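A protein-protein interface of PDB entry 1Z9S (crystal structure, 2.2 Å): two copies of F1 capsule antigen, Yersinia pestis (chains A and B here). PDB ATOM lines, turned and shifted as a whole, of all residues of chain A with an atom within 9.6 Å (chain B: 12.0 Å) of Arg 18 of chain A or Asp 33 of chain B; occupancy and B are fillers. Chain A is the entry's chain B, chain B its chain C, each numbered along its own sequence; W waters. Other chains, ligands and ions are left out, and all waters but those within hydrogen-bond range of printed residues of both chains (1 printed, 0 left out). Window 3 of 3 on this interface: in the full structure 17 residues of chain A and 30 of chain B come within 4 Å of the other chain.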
ATOM      1  N   VAL A  14     -27.154  -4.781  -8.433  1.00  0.00           N
ATOM      2  CA  VAL A  14     -27.183  -3.445  -9.008  1.00  0.00           C
ATOM      3  C   VAL A  14     -26.359  -3.318 -10.281  1.00  0.00           C
ATOM      4  O   VAL A  14     -25.377  -4.025 -10.484  1.00  0.00           O
ATOM      5  CB  VAL A  14     -26.676  -2.381  -7.996  1.00  0.00           C
ATOM      6  CG1 VAL A  14     -27.479  -2.461  -6.709  1.00  0.00           C
ATOM      7  CG2 VAL A  14     -25.195  -2.587  -7.706  1.00  0.00           C
ATOM      8  N   GLU A  15     -26.795  -2.412 -11.146  1.00  0.00           N
ATOM      9  CA  GLU A  15     -26.108  -2.127 -12.391  1.00  0.00           C
ATOM     10  C   GLU A  15     -25.524  -0.723 -12.220  1.00  0.00           C
ATOM     11  O   GLU A  15     -26.254   0.257 -12.117  1.00  0.00           O
ATOM     12  CB  GLU A  15     -27.089  -2.182 -13.579  1.00  0.00           C
ATOM     13  CG  GLU A  15     -27.308  -3.602 -14.131  1.00  0.00           C
ATOM     14  CD  GLU A  15     -28.382  -3.666 -15.205  1.00  0.00           C
ATOM     15  OE1 GLU A  15     -28.342  -2.854 -16.152  1.00  0.00           O
ATOM     16  OE2 GLU A  15     -29.271  -4.533 -15.102  1.00  0.00           O
ATOM     17  N   PRO A  16     -24.189  -0.616 -12.174  1.00  0.00           N
ATOM     18  CA  PRO A  16     -23.530   0.680 -12.006  1.00  0.00           C
ATOM     19  C   PRO A  16     -23.664   1.537 -13.262  1.00  0.00           C
ATOM     20  O   PRO A  16     -24.108   1.055 -14.311  1.00  0.00           O
ATOM     21  CB  PRO A  16     -22.064   0.307 -11.744  1.00  0.00           C
ATOM     22  CG  PRO A  16     -22.068  -1.193 -11.517  1.00  0.00           C
ATOM     23  CD  PRO A  16     -23.194  -1.682 -12.369  1.00  0.00           C
ATOM     24  N   ALA A  17     -23.268   2.803 -13.149  1.00  0.00           N
ATOM     25  CA  ALA A  17     -23.305   3.716 -14.283  1.00  0.00           C
ATOM     26  C   ALA A  17     -21.875   3.859 -14.783  1.00  0.00           C
ATOM     27  O   ALA A  17     -21.097   4.636 -14.228  1.00  0.00           O
ATOM     28  CB  ALA A  17     -23.846   5.068 -13.861  1.00  0.00           C
ATOM     29  N   ARG A  18     -21.541   3.098 -15.821  1.00  0.00           N
ATOM     30  CA  ARG A  18     -20.211   3.123 -16.411  1.00  0.00           C
ATOM     31  C   ARG A  18     -20.175   3.956 -17.675  1.00  0.00           C
ATOM     32  O   ARG A  18     -21.009   3.784 -18.564  1.00  0.00           O
ATOM     33  CB  ARG A  18     -19.749   1.715 -16.785  1.00  0.00           C
ATOM     34  CG  ARG A  18     -19.856   0.676 -15.702  1.00  0.00           C
ATOM     35  CD  ARG A  18     -19.005  -0.530 -16.070  1.00  0.00           C
ATOM     36  NE  ARG A  18     -19.175  -1.607 -15.100  1.00  0.00           N
ATOM     37  CZ  ARG A  18     -20.269  -2.352 -15.012  1.00  0.00           C
ATOM     38  NH1 ARG A  18     -21.279  -2.132 -15.845  1.00  0.00           N
ATOM     39  NH2 ARG A  18     -20.363  -3.294 -14.081  1.00  0.00           N
ATOM     40  N   ILE A  19     -19.198   4.849 -17.764  1.00  0.00           N
ATOM     41  CA  ILE A  19     -19.043   5.672 -18.950  1.00  0.00           C
ATOM     42  C   ILE A  19     -17.573   5.685 -19.339  1.00  0.00           C
ATOM     43  O   ILE A  19     -16.701   5.926 -18.499  1.00  0.00           O
ATOM     44  CB  ILE A  19     -19.490   7.129 -18.715  1.00  0.00           C
ATOM     45  CG1 ILE A  19     -20.944   7.166 -18.231  1.00  0.00           C
ATOM     46  CG2 ILE A  19     -19.337   7.926 -20.013  1.00  0.00           C
ATOM     47  CD1 ILE A  19     -21.956   6.680 -19.270  1.00  0.00           C
ATOM     48  N   THR A  20     -17.292   5.396 -20.604  1.00  0.00           N
ATOM     49  CA  THR A  20     -15.917   5.421 -21.081  1.00  0.00           C
ATOM     50  C   THR A  20     -15.861   6.230 -22.357  1.00  0.00           C
ATOM     51  O   THR A  20     -16.872   6.407 -23.042  1.00  0.00           O
ATOM     52  CB  THR A  20     -15.364   4.008 -21.384  1.00  0.00           C
ATOM     53  OG1 THR A  20     -16.152   3.394 -22.410  1.00  0.00           O
ATOM     54  CG2 THR A  20     -15.376   3.137 -20.109  1.00  0.00           C
ATOM     55  N   LEU A  21     -14.679   6.739 -22.668  1.00  0.00           N
ATOM     56  CA  LEU A  21     -14.498   7.512 -23.881  1.00  0.00           C
ATOM     57  C   LEU A  21     -13.123   7.206 -24.443  1.00  0.00           C
ATOM     58  O   LEU A  21     -12.143   7.104 -23.702  1.00  0.00           O
ATOM     59  CB  LEU A  21     -14.621   9.014 -23.600  1.00  0.00           C
ATOM     60  CG  LEU A  21     -14.568   9.885 -24.863  1.00  0.00           C
ATOM     61  CD1 LEU A  21     -15.873   9.726 -25.634  1.00  0.00           C
ATOM     62  CD2 LEU A  21     -14.349  11.340 -24.503  1.00  0.00           C
ATOM     63  N   LEU A  48     -17.843   6.533 -27.548  1.00  0.00           N
ATOM     64  CA  LEU A  48     -18.451   6.581 -26.225  1.00  0.00           C
ATOM     65  C   LEU A  48     -18.918   5.180 -25.891  1.00  0.00           C
ATOM     66  O   LEU A  48     -19.566   4.532 -26.710  1.00  0.00           O
ATOM     67  CB  LEU A  48     -19.657   7.524 -26.230  1.00  0.00           C
ATOM     68  CG  LEU A  48     -20.431   7.666 -24.918  1.00  0.00           C
ATOM     69  CD1 LEU A  48     -19.570   8.395 -23.890  1.00  0.00           C
ATOM     70  CD2 LEU A  48     -21.711   8.445 -25.164  1.00  0.00           C
ATOM     71  N   GLY A  49     -18.598   4.706 -24.694  1.00  0.00           N
ATOM     72  CA  GLY A  49     -19.025   3.369 -24.320  1.00  0.00           C
ATOM     73  C   GLY A  49     -19.400   3.239 -22.855  1.00  0.00           C
ATOM     74  O   GLY A  49     -19.423   4.228 -22.112  1.00  0.00           O
ATOM     75  N   GLY A  50     -19.699   2.007 -22.451  1.00  0.00           N
ATOM     76  CA  GLY A  50     -20.045   1.725 -21.072  1.00  0.00           C
ATOM     77  C   GLY A  50     -21.512   1.856 -20.727  1.00  0.00           C
ATOM     78  O   GLY A  50     -22.048   1.030 -19.983  1.00  0.00           O
ATOM     79  N   TYR A  51     -22.167   2.880 -21.273  1.00  0.00           N
ATOM     80  CA  TYR A  51     -23.580   3.138 -20.985  1.00  0.00           C
ATOM     81  C   TYR A  51     -24.520   1.960 -21.210  1.00  0.00           C
ATOM     82  O   TYR A  51     -24.249   1.067 -22.016  1.00  0.00           O
ATOM     83  CB  TYR A  51     -24.076   4.332 -21.804  1.00  0.00           C
ATOM     84  CG  TYR A  51     -23.954   4.150 -23.304  1.00  0.00           C
ATOM     85  CD1 TYR A  51     -24.847   3.337 -24.013  1.00  0.00           C
ATOM     86  CD2 TYR A  51     -22.925   4.770 -24.010  1.00  0.00           C
ATOM     87  CE1 TYR A  51     -24.710   3.150 -25.396  1.00  0.00           C
ATOM     88  CE2 TYR A  51     -22.777   4.591 -25.383  1.00  0.00           C
ATOM     89  CZ  TYR A  51     -23.668   3.783 -26.070  1.00  0.00           C
ATOM     90  OH  TYR A  51     -23.492   3.607 -27.422  1.00  0.00           O
ATOM     91  N   LYS A  52     -25.635   1.983 -20.488  1.00  0.00           N
ATOM     92  CA  LYS A  52     -26.647   0.948 -20.581  1.00  0.00           C
ATOM     93  C   LYS A  52     -27.478   1.139 -21.855  1.00  0.00           C
ATOM     94  O   LYS A  52     -27.798   2.273 -22.239  1.00  0.00           O
ATOM     95  CB  LYS A  52     -27.560   1.011 -19.347  1.00  0.00           C
ATOM     96  CG  LYS A  52     -28.672  -0.034 -19.334  1.00  0.00           C
ATOM     97  CD  LYS A  52     -29.407  -0.050 -17.992  1.00  0.00           C
ATOM     98  CE  LYS A  52     -30.393  -1.216 -17.912  1.00  0.00           C
ATOM     99  NZ  LYS A  52     -29.733  -2.498 -18.296  1.00  0.00           N
ATOM    100  N   THR A  53     -27.826   0.029 -22.503  1.00  0.00           N
ATOM    101  CA  THR A  53     -28.624   0.077 -23.719  1.00  0.00           C
ATOM    102  C   THR A  53     -29.895   0.873 -23.428  1.00  0.00           C
ATOM    103  O   THR A  53     -30.639   0.567 -22.491  1.00  0.00           O
ATOM    104  CB  THR A  53     -28.997  -1.355 -24.201  1.00  0.00           C
ATOM    105  OG1 THR A  53     -27.803  -2.120 -24.401  1.00  0.00           O
ATOM    106  CG2 THR A  53     -29.770  -1.299 -25.522  1.00  0.00           C
ATOM    107  N   THR A  55     -29.545   4.397 -23.595  1.00  0.00           N
ATOM    108  CA  THR A  55     -28.963   5.724 -23.461  1.00  0.00           C
ATOM    109  C   THR A  55     -29.282   6.488 -24.742  1.00  0.00           C
ATOM    110  O   THR A  55     -29.126   5.955 -25.845  1.00  0.00           O
ATOM    111  CB  THR A  55     -27.449   5.628 -23.279  1.00  0.00           C
ATOM    112  OG1 THR A  55     -27.169   4.985 -22.033  1.00  0.00           O
ATOM    113  CG2 THR A  55     -26.810   7.011 -23.287  1.00  0.00           C
ATOM    114  N   THR A 116     -25.947  -0.017 -29.484  1.00  0.00           N
ATOM    115  CA  THR A 116     -25.719  -0.890 -28.342  1.00  0.00           C
ATOM    116  C   THR A 116     -24.227  -1.076 -28.093  1.00  0.00           C
ATOM    117  O   THR A 116     -23.454  -1.249 -29.031  1.00  0.00           O
ATOM    118  CB  THR A 116     -26.356  -2.270 -28.575  1.00  0.00           C
ATOM    119  OG1 THR A 116     -27.769  -2.118 -28.751  1.00  0.00           O
ATOM    120  CG2 THR A 116     -26.097  -3.186 -27.389  1.00  0.00           C
ATOM    121  N   GLY A 117     -23.824  -1.034 -26.828  1.00  0.00           N
ATOM    122  CA  GLY A 117     -22.420  -1.211 -26.497  1.00  0.00           C
ATOM    123  C   GLY A 117     -21.598   0.067 -26.546  1.00  0.00           C
ATOM    124  O   GLY A 117     -21.102   0.540 -25.521  1.00  0.00           O
ATOM    125  N   SER A 118     -21.428   0.624 -27.740  1.00  0.00           N
ATOM    126  CA  SER A 118     -20.659   1.853 -27.896  1.00  0.00           C
ATOM    127  C   SER A 118     -21.153   2.607 -29.115  1.00  0.00           C
ATOM    128  O   SER A 118     -21.781   2.025 -30.006  1.00  0.00           O
ATOM    129  CB  SER A 118     -19.167   1.553 -28.052  1.00  0.00           C
ATOM    130  OG  SER A 118     -18.921   0.805 -29.229  1.00  0.00           O
ATOM    131  N   VAL A 146     -22.856  12.874 -19.589  1.00  0.00           N
ATOM    132  CA  VAL A 146     -23.875  11.892 -19.922  1.00  0.00           C
ATOM    133  C   VAL A 146     -24.860  11.824 -18.769  1.00  0.00           C
ATOM    134  O   VAL A 146     -24.479  11.593 -17.614  1.00  0.00           O
ATOM    135  CB  VAL A 146     -23.291  10.480 -20.119  1.00  0.00           C
ATOM    136  CG1 VAL A 146     -24.396   9.528 -20.558  1.00  0.00           C
ATOM    137  CG2 VAL A 146     -22.144  10.506 -21.140  1.00  0.00           C
ATOM    138  N   ASN A 148     -27.466   9.675 -17.435  1.00  0.00           N
ATOM    139  CA  ASN A 148     -28.016   8.331 -17.496  1.00  0.00           C
ATOM    140  C   ASN A 148     -29.509   8.263 -17.175  1.00  0.00           C
ATOM    141  O   ASN A 148     -30.003   8.998 -16.318  1.00  0.00           O
ATOM    142  CB  ASN A 148     -27.239   7.414 -16.538  1.00  0.00           C
ATOM    143  CG  ASN A 148     -25.770   7.284 -16.914  1.00  0.00           C
ATOM    144  OD1 ASN A 148     -25.427   6.585 -17.858  1.00  0.00           O
ATOM    145  ND2 ASN A 148     -24.900   7.972 -16.181  1.00  0.00           N
ATOM    146  N   PRO B  28     -24.769  -5.232  -1.469  1.00  0.00           N
ATOM    147  CA  PRO B  28     -25.371  -5.278  -2.805  1.00  0.00           C
ATOM    148  C   PRO B  28     -24.406  -5.977  -3.761  1.00  0.00           C
ATOM    149  O   PRO B  28     -23.192  -5.877  -3.594  1.00  0.00           O
ATOM    150  CB  PRO B  28     -25.531  -3.798  -3.153  1.00  0.00           C
ATOM    151  CG  PRO B  28     -25.796  -3.171  -1.811  1.00  0.00           C
ATOM    152  CD  PRO B  28     -24.771  -3.856  -0.935  1.00  0.00           C
ATOM    153  N   ILE B  29     -24.939  -6.684  -4.754  1.00  0.00           N
ATOM    154  CA  ILE B  29     -24.099  -7.377  -5.731  1.00  0.00           C
ATOM    155  C   ILE B  29     -24.004  -6.550  -7.023  1.00  0.00           C
ATOM    156  O   ILE B  29     -25.015  -6.275  -7.679  1.00  0.00           O
ATOM    157  CB  ILE B  29     -24.674  -8.776  -6.096  1.00  0.00           C
ATOM    158  CG1 ILE B  29     -24.912  -9.618  -4.829  1.00  0.00           C
ATOM    159  CG2 ILE B  29     -23.726  -9.494  -7.064  1.00  0.00           C
ATOM    160  CD1 ILE B  29     -23.695  -9.789  -3.953  1.00  0.00           C
ATOM    161  N   THR B  30     -22.789  -6.157  -7.395  1.00  0.00           N
ATOM    162  CA  THR B  30     -22.600  -5.363  -8.608  1.00  0.00           C
ATOM    163  C   THR B  30     -22.561  -6.246  -9.864  1.00  0.00           C
ATOM    164  O   THR B  30     -21.744  -7.163  -9.954  1.00  0.00           O
ATOM    165  CB  THR B  30     -21.292  -4.535  -8.531  1.00  0.00           C
ATOM    166  OG1 THR B  30     -21.360  -3.627  -7.419  1.00  0.00           O
ATOM    167  CG2 THR B  30     -21.095  -3.726  -9.807  1.00  0.00           C
ATOM    168  N   ILE B  31     -23.453  -5.987 -10.820  1.00  0.00           N
ATOM    169  CA  ILE B  31     -23.471  -6.760 -12.064  1.00  0.00           C
ATOM    170  C   ILE B  31     -22.331  -6.239 -12.931  1.00  0.00           C
ATOM    171  O   ILE B  31     -22.208  -5.029 -13.130  1.00  0.00           O
ATOM    172  CB  ILE B  31     -24.778  -6.561 -12.873  1.00  0.00           C
ATOM    173  CG1 ILE B  31     -26.005  -6.949 -12.036  1.00  0.00           C
ATOM    174  CG2 ILE B  31     -24.724  -7.397 -14.152  1.00  0.00           C
ATOM    175  CD1 ILE B  31     -26.070  -8.403 -11.704  1.00  0.00           C
ATOM    176  N   MET B  32     -21.496  -7.141 -13.434  1.00  0.00           N
ATOM    177  CA  MET B  32     -20.375  -6.747 -14.282  1.00  0.00           C
ATOM    178  C   MET B  32     -20.901  -6.339 -15.656  1.00  0.00           C
ATOM    179  O   MET B  32     -22.066  -6.581 -15.980  1.00  0.00           O
ATOM    180  CB  MET B  32     -19.397  -7.909 -14.433  1.00  0.00           C
ATOM    181  CG  MET B  32     -19.046  -8.577 -13.132  1.00  0.00           C
ATOM    182  SD  MET B  32     -17.969 -10.011 -13.376  1.00  0.00           S
ATOM    183  CE  MET B  32     -16.627  -9.578 -12.277  1.00  0.00           C
ATOM    184  N   ASP B  33     -20.045  -5.731 -16.471  1.00  0.00           N
ATOM    185  CA  ASP B  33     -20.461  -5.299 -17.803  1.00  0.00           C
ATOM    186  C   ASP B  33     -20.941  -6.454 -18.674  1.00  0.00           C
ATOM    187  O   ASP B  33     -21.827  -6.272 -19.515  1.00  0.00           O
ATOM    188  CB  ASP B  33     -19.325  -4.573 -18.526  1.00  0.00           C
ATOM    189  CG  ASP B  33     -19.726  -4.128 -19.925  1.00  0.00           C
ATOM    190  OD1 ASP B  33     -19.105  -4.596 -20.904  1.00  0.00           O
ATOM    191  OD2 ASP B  33     -20.672  -3.321 -20.046  1.00  0.00           O
ATOM    192  N   ASN B  34     -20.366  -7.638 -18.478  1.00  0.00           N
ATOM    193  CA  ASN B  34     -20.766  -8.804 -19.266  1.00  0.00           C
ATOM    194  C   ASN B  34     -22.059  -9.434 -18.740  1.00  0.00           C
ATOM    195  O   ASN B  34     -22.514 -10.475 -19.239  1.00  0.00           O
ATOM    196  CB  ASN B  34     -19.638  -9.842 -19.291  1.00  0.00           C
ATOM    197  CG  ASN B  34     -19.400 -10.476 -17.945  1.00  0.00           C
ATOM    198  OD1 ASN B  34     -19.980 -10.066 -16.938  1.00  0.00           O
ATOM    199  ND2 ASN B  34     -18.537 -11.488 -17.914  1.00  0.00           N
ATOM    200  N   GLY B  35     -22.648  -8.801 -17.729  1.00  0.00           N
ATOM    201  CA  GLY B  35     -23.893  -9.303 -17.172  1.00  0.00           C
ATOM    202  C   GLY B  35     -23.793 -10.457 -16.190  1.00  0.00           C
ATOM    203  O   GLY B  35     -24.820 -11.040 -15.825  1.00  0.00           O
ATOM    204  N   ASN B  36     -22.577 -10.798 -15.766  1.00  0.00           N
ATOM    205  CA  ASN B  36     -22.374 -11.885 -14.806  1.00  0.00           C
ATOM    206  C   ASN B  36     -21.977 -11.210 -13.500  1.00  0.00           C
ATOM    207  O   ASN B  36     -21.907  -9.980 -13.425  1.00  0.00           O
ATOM    208  CB  ASN B  36     -21.229 -12.803 -15.258  1.00  0.00           C
ATOM    209  CG  ASN B  36     -21.379 -14.253 -14.762  1.00  0.00           C
ATOM    210  OD1 ASN B  36     -22.016 -14.532 -13.742  1.00  0.00           O
ATOM    211  ND2 ASN B  36     -20.767 -15.178 -15.492  1.00  0.00           N
ATOM    212  N   ILE B  37     -21.733 -12.004 -12.468  1.00  0.00           N
ATOM    213  CA  ILE B  37     -21.321 -11.457 -11.187  1.00  0.00           C
ATOM    214  C   ILE B  37     -20.053 -12.190 -10.814  1.00  0.00           C
ATOM    215  O   ILE B  37     -19.724 -13.215 -11.402  1.00  0.00           O
ATOM    216  CB  ILE B  37     -22.372 -11.670 -10.065  1.00  0.00           C
ATOM    217  CG1 ILE B  37     -22.726 -13.152  -9.945  1.00  0.00           C
ATOM    218  CG2 ILE B  37     -23.606 -10.792 -10.312  1.00  0.00           C
ATOM    219  CD1 ILE B  37     -23.681 -13.450  -8.813  1.00  0.00           C
ATOM    220  N   ASP B  38     -19.340 -11.659  -9.834  1.00  0.00           N
ATOM    221  CA  ASP B  38     -18.091 -12.250  -9.403  1.00  0.00           C
ATOM    222  C   ASP B  38     -18.352 -13.413  -8.437  1.00  0.00           C
ATOM    223  O   ASP B  38     -19.451 -13.544  -7.892  1.00  0.00           O
ATOM    224  CB  ASP B  38     -17.244 -11.158  -8.750  1.00  0.00           C
ATOM    225  CG  ASP B  38     -15.803 -11.572  -8.553  1.00  0.00           C
ATOM    226  OD1 ASP B  38     -15.427 -12.673  -9.002  1.00  0.00           O
ATOM    227  OD2 ASP B  38     -15.045 -10.786  -7.949  1.00  0.00           O
ATOM    228  N   LEU B  41     -18.409 -13.760  -3.461  1.00  0.00           N
ATOM    229  CA  LEU B  41     -19.036 -12.625  -2.787  1.00  0.00           C
ATOM    230  C   LEU B  41     -19.961 -13.144  -1.681  1.00  0.00           C
ATOM    231  O   LEU B  41     -20.573 -14.210  -1.819  1.00  0.00           O
ATOM    232  CB  LEU B  41     -19.865 -11.815  -3.779  1.00  0.00           C
ATOM    233  CG  LEU B  41     -19.144 -11.323  -5.035  1.00  0.00           C
ATOM    234  CD1 LEU B  41     -20.158 -10.681  -5.978  1.00  0.00           C
ATOM    235  CD2 LEU B  41     -18.058 -10.321  -4.644  1.00  0.00           C
ATOM    236  N   SER B 128     -23.932 -16.418 -12.573  1.00  0.00           N
ATOM    237  CA  SER B 128     -25.197 -16.483 -13.299  1.00  0.00           C
ATOM    238  C   SER B 128     -25.466 -17.906 -13.795  1.00  0.00           C
ATOM    239  O   SER B 128     -24.540 -18.651 -14.083  1.00  0.00           O
ATOM    240  CB  SER B 128     -25.140 -15.534 -14.505  1.00  0.00           C
ATOM    241  OG  SER B 128     -26.303 -15.636 -15.299  1.00  0.00           O
ATOM    242  N   GLY B 131     -26.937 -16.351 -19.390  1.00  0.00           N
ATOM    243  CA  GLY B 131     -27.466 -15.076 -19.837  1.00  0.00           C
ATOM    244  C   GLY B 131     -27.083 -13.973 -18.869  1.00  0.00           C
ATOM    245  O   GLY B 131     -26.630 -14.242 -17.755  1.00  0.00           O
ATOM    246  N   LYS B 132     -27.260 -12.729 -19.292  1.00  0.00           N
ATOM    247  CA  LYS B 132     -26.909 -11.589 -18.458  1.00  0.00           C
ATOM    248  C   LYS B 132     -27.968 -11.374 -17.381  1.00  0.00           C
ATOM    249  O   LYS B 132     -29.159 -11.542 -17.625  1.00  0.00           O
ATOM    250  CB  LYS B 132     -26.768 -10.333 -19.326  1.00  0.00           C
ATOM    251  CG  LYS B 132     -25.812 -10.513 -20.501  1.00  0.00           C
ATOM    252  CD  LYS B 132     -25.804  -9.295 -21.425  1.00  0.00           C
ATOM    253  CE  LYS B 132     -25.329  -8.037 -20.702  1.00  0.00           C
ATOM    254  NZ  LYS B 132     -25.213  -6.877 -21.635  1.00  0.00           N
ATOM    255  N   LEU B 133     -27.518 -11.007 -16.186  1.00  0.00           N
ATOM    256  CA  LEU B 133     -28.421 -10.769 -15.071  1.00  0.00           C
ATOM    257  C   LEU B 133     -28.926  -9.322 -15.104  1.00  0.00           C
ATOM    258  O   LEU B 133     -28.213  -8.414 -15.516  1.00  0.00           O
ATOM    259  CB  LEU B 133     -27.703 -11.056 -13.743  1.00  0.00           C
ATOM    260  CG  LEU B 133     -27.157 -12.487 -13.533  1.00  0.00           C
ATOM    261  CD1 LEU B 133     -26.420 -12.556 -12.205  1.00  0.00           C
ATOM    262  CD2 LEU B 133     -28.297 -13.522 -13.551  1.00  0.00           C
ATOM    263  N   ALA B 134     -30.174  -9.126 -14.693  1.00  0.00           N
ATOM    264  CA  ALA B 134     -30.781  -7.801 -14.641  1.00  0.00           C
ATOM    265  C   ALA B 134     -30.754  -7.353 -13.180  1.00  0.00           C
ATOM    266  O   ALA B 134     -30.998  -8.154 -12.279  1.00  0.00           O
ATOM    267  CB  ALA B 134     -32.224  -7.861 -15.146  1.00  0.00           C
ATOM    268  N   ALA B 135     -30.448  -6.084 -12.943  1.00  0.00           N
ATOM    269  CA  ALA B 135     -30.403  -5.570 -11.579  1.00  0.00           C
ATOM    270  C   ALA B 135     -31.796  -5.634 -10.948  1.00  0.00           C
ATOM    271  O   ALA B 135     -32.806  -5.505 -11.643  1.00  0.00           O
ATOM    272  CB  ALA B 135     -29.893  -4.136 -11.582  1.00  0.00           C
HETATM  273  O   HOH W   1     -23.978  -3.888 -15.506  1.00  0.00           O
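Water W1 lies within hydrogen-bond range of the backbone carbonyl oxygen (O) of Ile 31 of chain B, the guanidinium group (NH1) of Arg 18 of chain A and the backbone carbonyl oxygen (O) of Met 32 of chain B.
Arg 18 of chain A touches just these residues of chain B: Ile 31 (2.7 Å), Met 32 (3.5 Å) and Asp 33 (3.4 Å).
Of chain A, only Arg 18 comes within 4 Å of Asp 33 of chain B.
Of chain B, only Thr 30 (3.2 Å) and Ile 31 (3.6 Å) come within 4 Å of Pro 16 of chain A.
Ala 17 of chain A touches none of the printed residues of chain B.
No residue of chain B comes within 4 Å of Gly 50 of chain A.
Of the printed residues of chain A, Ile 31 of chain B touches Val 14, Pro 16 and Arg 18.
Of the printed residues of chain B, Glu 15 of chain A touches Ala 134 and Ala 135.
Printed residues of chain A within 4 Å of Met 32 of chain B: Arg 18 (3.5 Å).
Of the printed residues of chain A, Thr 30 of chain B touches Val 14 and Pro 16.
The nearest residue of chain B that does not touch Arg 18 of chain A is Thr 30 of chain B (4.4 Å).
No position is printed for both chains.
Among the printed residues, merely in contact across the chains: Val 14 of chain A with Thr 30 of chain B (3.6 Å), Val 14 of chain A with Ala 135 of chain B (3.8 Å), Glu 15 of chain A with Ala 134 of chain B (3.6 Å), Pro 16 of chain A with Thr 30 of chain B (3.2 Å), Pro 16 of chain A with Ile 31 of chain B (3.6 Å) and Arg 18 of chain A with Met 32 of chain B (3.5 Å).
The side-chain carboxylate (OE1) of Glu 15 of chain A lies within salt-bridge range of the side-chain amino group (NZ) of Lys 52 of chain A (2.6 Å).
The backbone carbonyl oxygen (O) of Arg 18 of chain A lies within hydrogen-bond range of the backbone NH (N) of Tyr 51 of chain A.
Hydrophobic or aromatic side chains of chain B within 4 Å of the printed part of chain A: Ile 31 and Ala 135.
Of the 20 printed residues of chain A, 4 touch a printed residue of chain B.
Hydrophobic or aromatic side chains of chain A that line the printed part of chain B: Val 14 and Pro 16.
N of Val 14 of chain A lies within hydrogen-bond range of O of Ile 29 of chain B, 2.7 Å away.
The backbone NH of Ile 31 of chain B is in hydrogen-bond range of the backbone carbonyl oxygen of Val 14 of chain A, 2.8 Å away.
The backbone NH (N) of Ala 135 of chain B sits at hydrogen-bond distance from the side-chain carboxylate (OE2) of Glu 15 of chain A (2.9 Å).
The guanidinium group of Arg 18 of chain A is in hydrogen-bond range of the backbone carbonyl oxygen of Ile 31 of chain B (2.7 Å).
The backbone NH (N) of Asp 33 of chain B sits close to the guanidinium group (NH2) of Arg 18 of chain A, 3.4 Å away.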
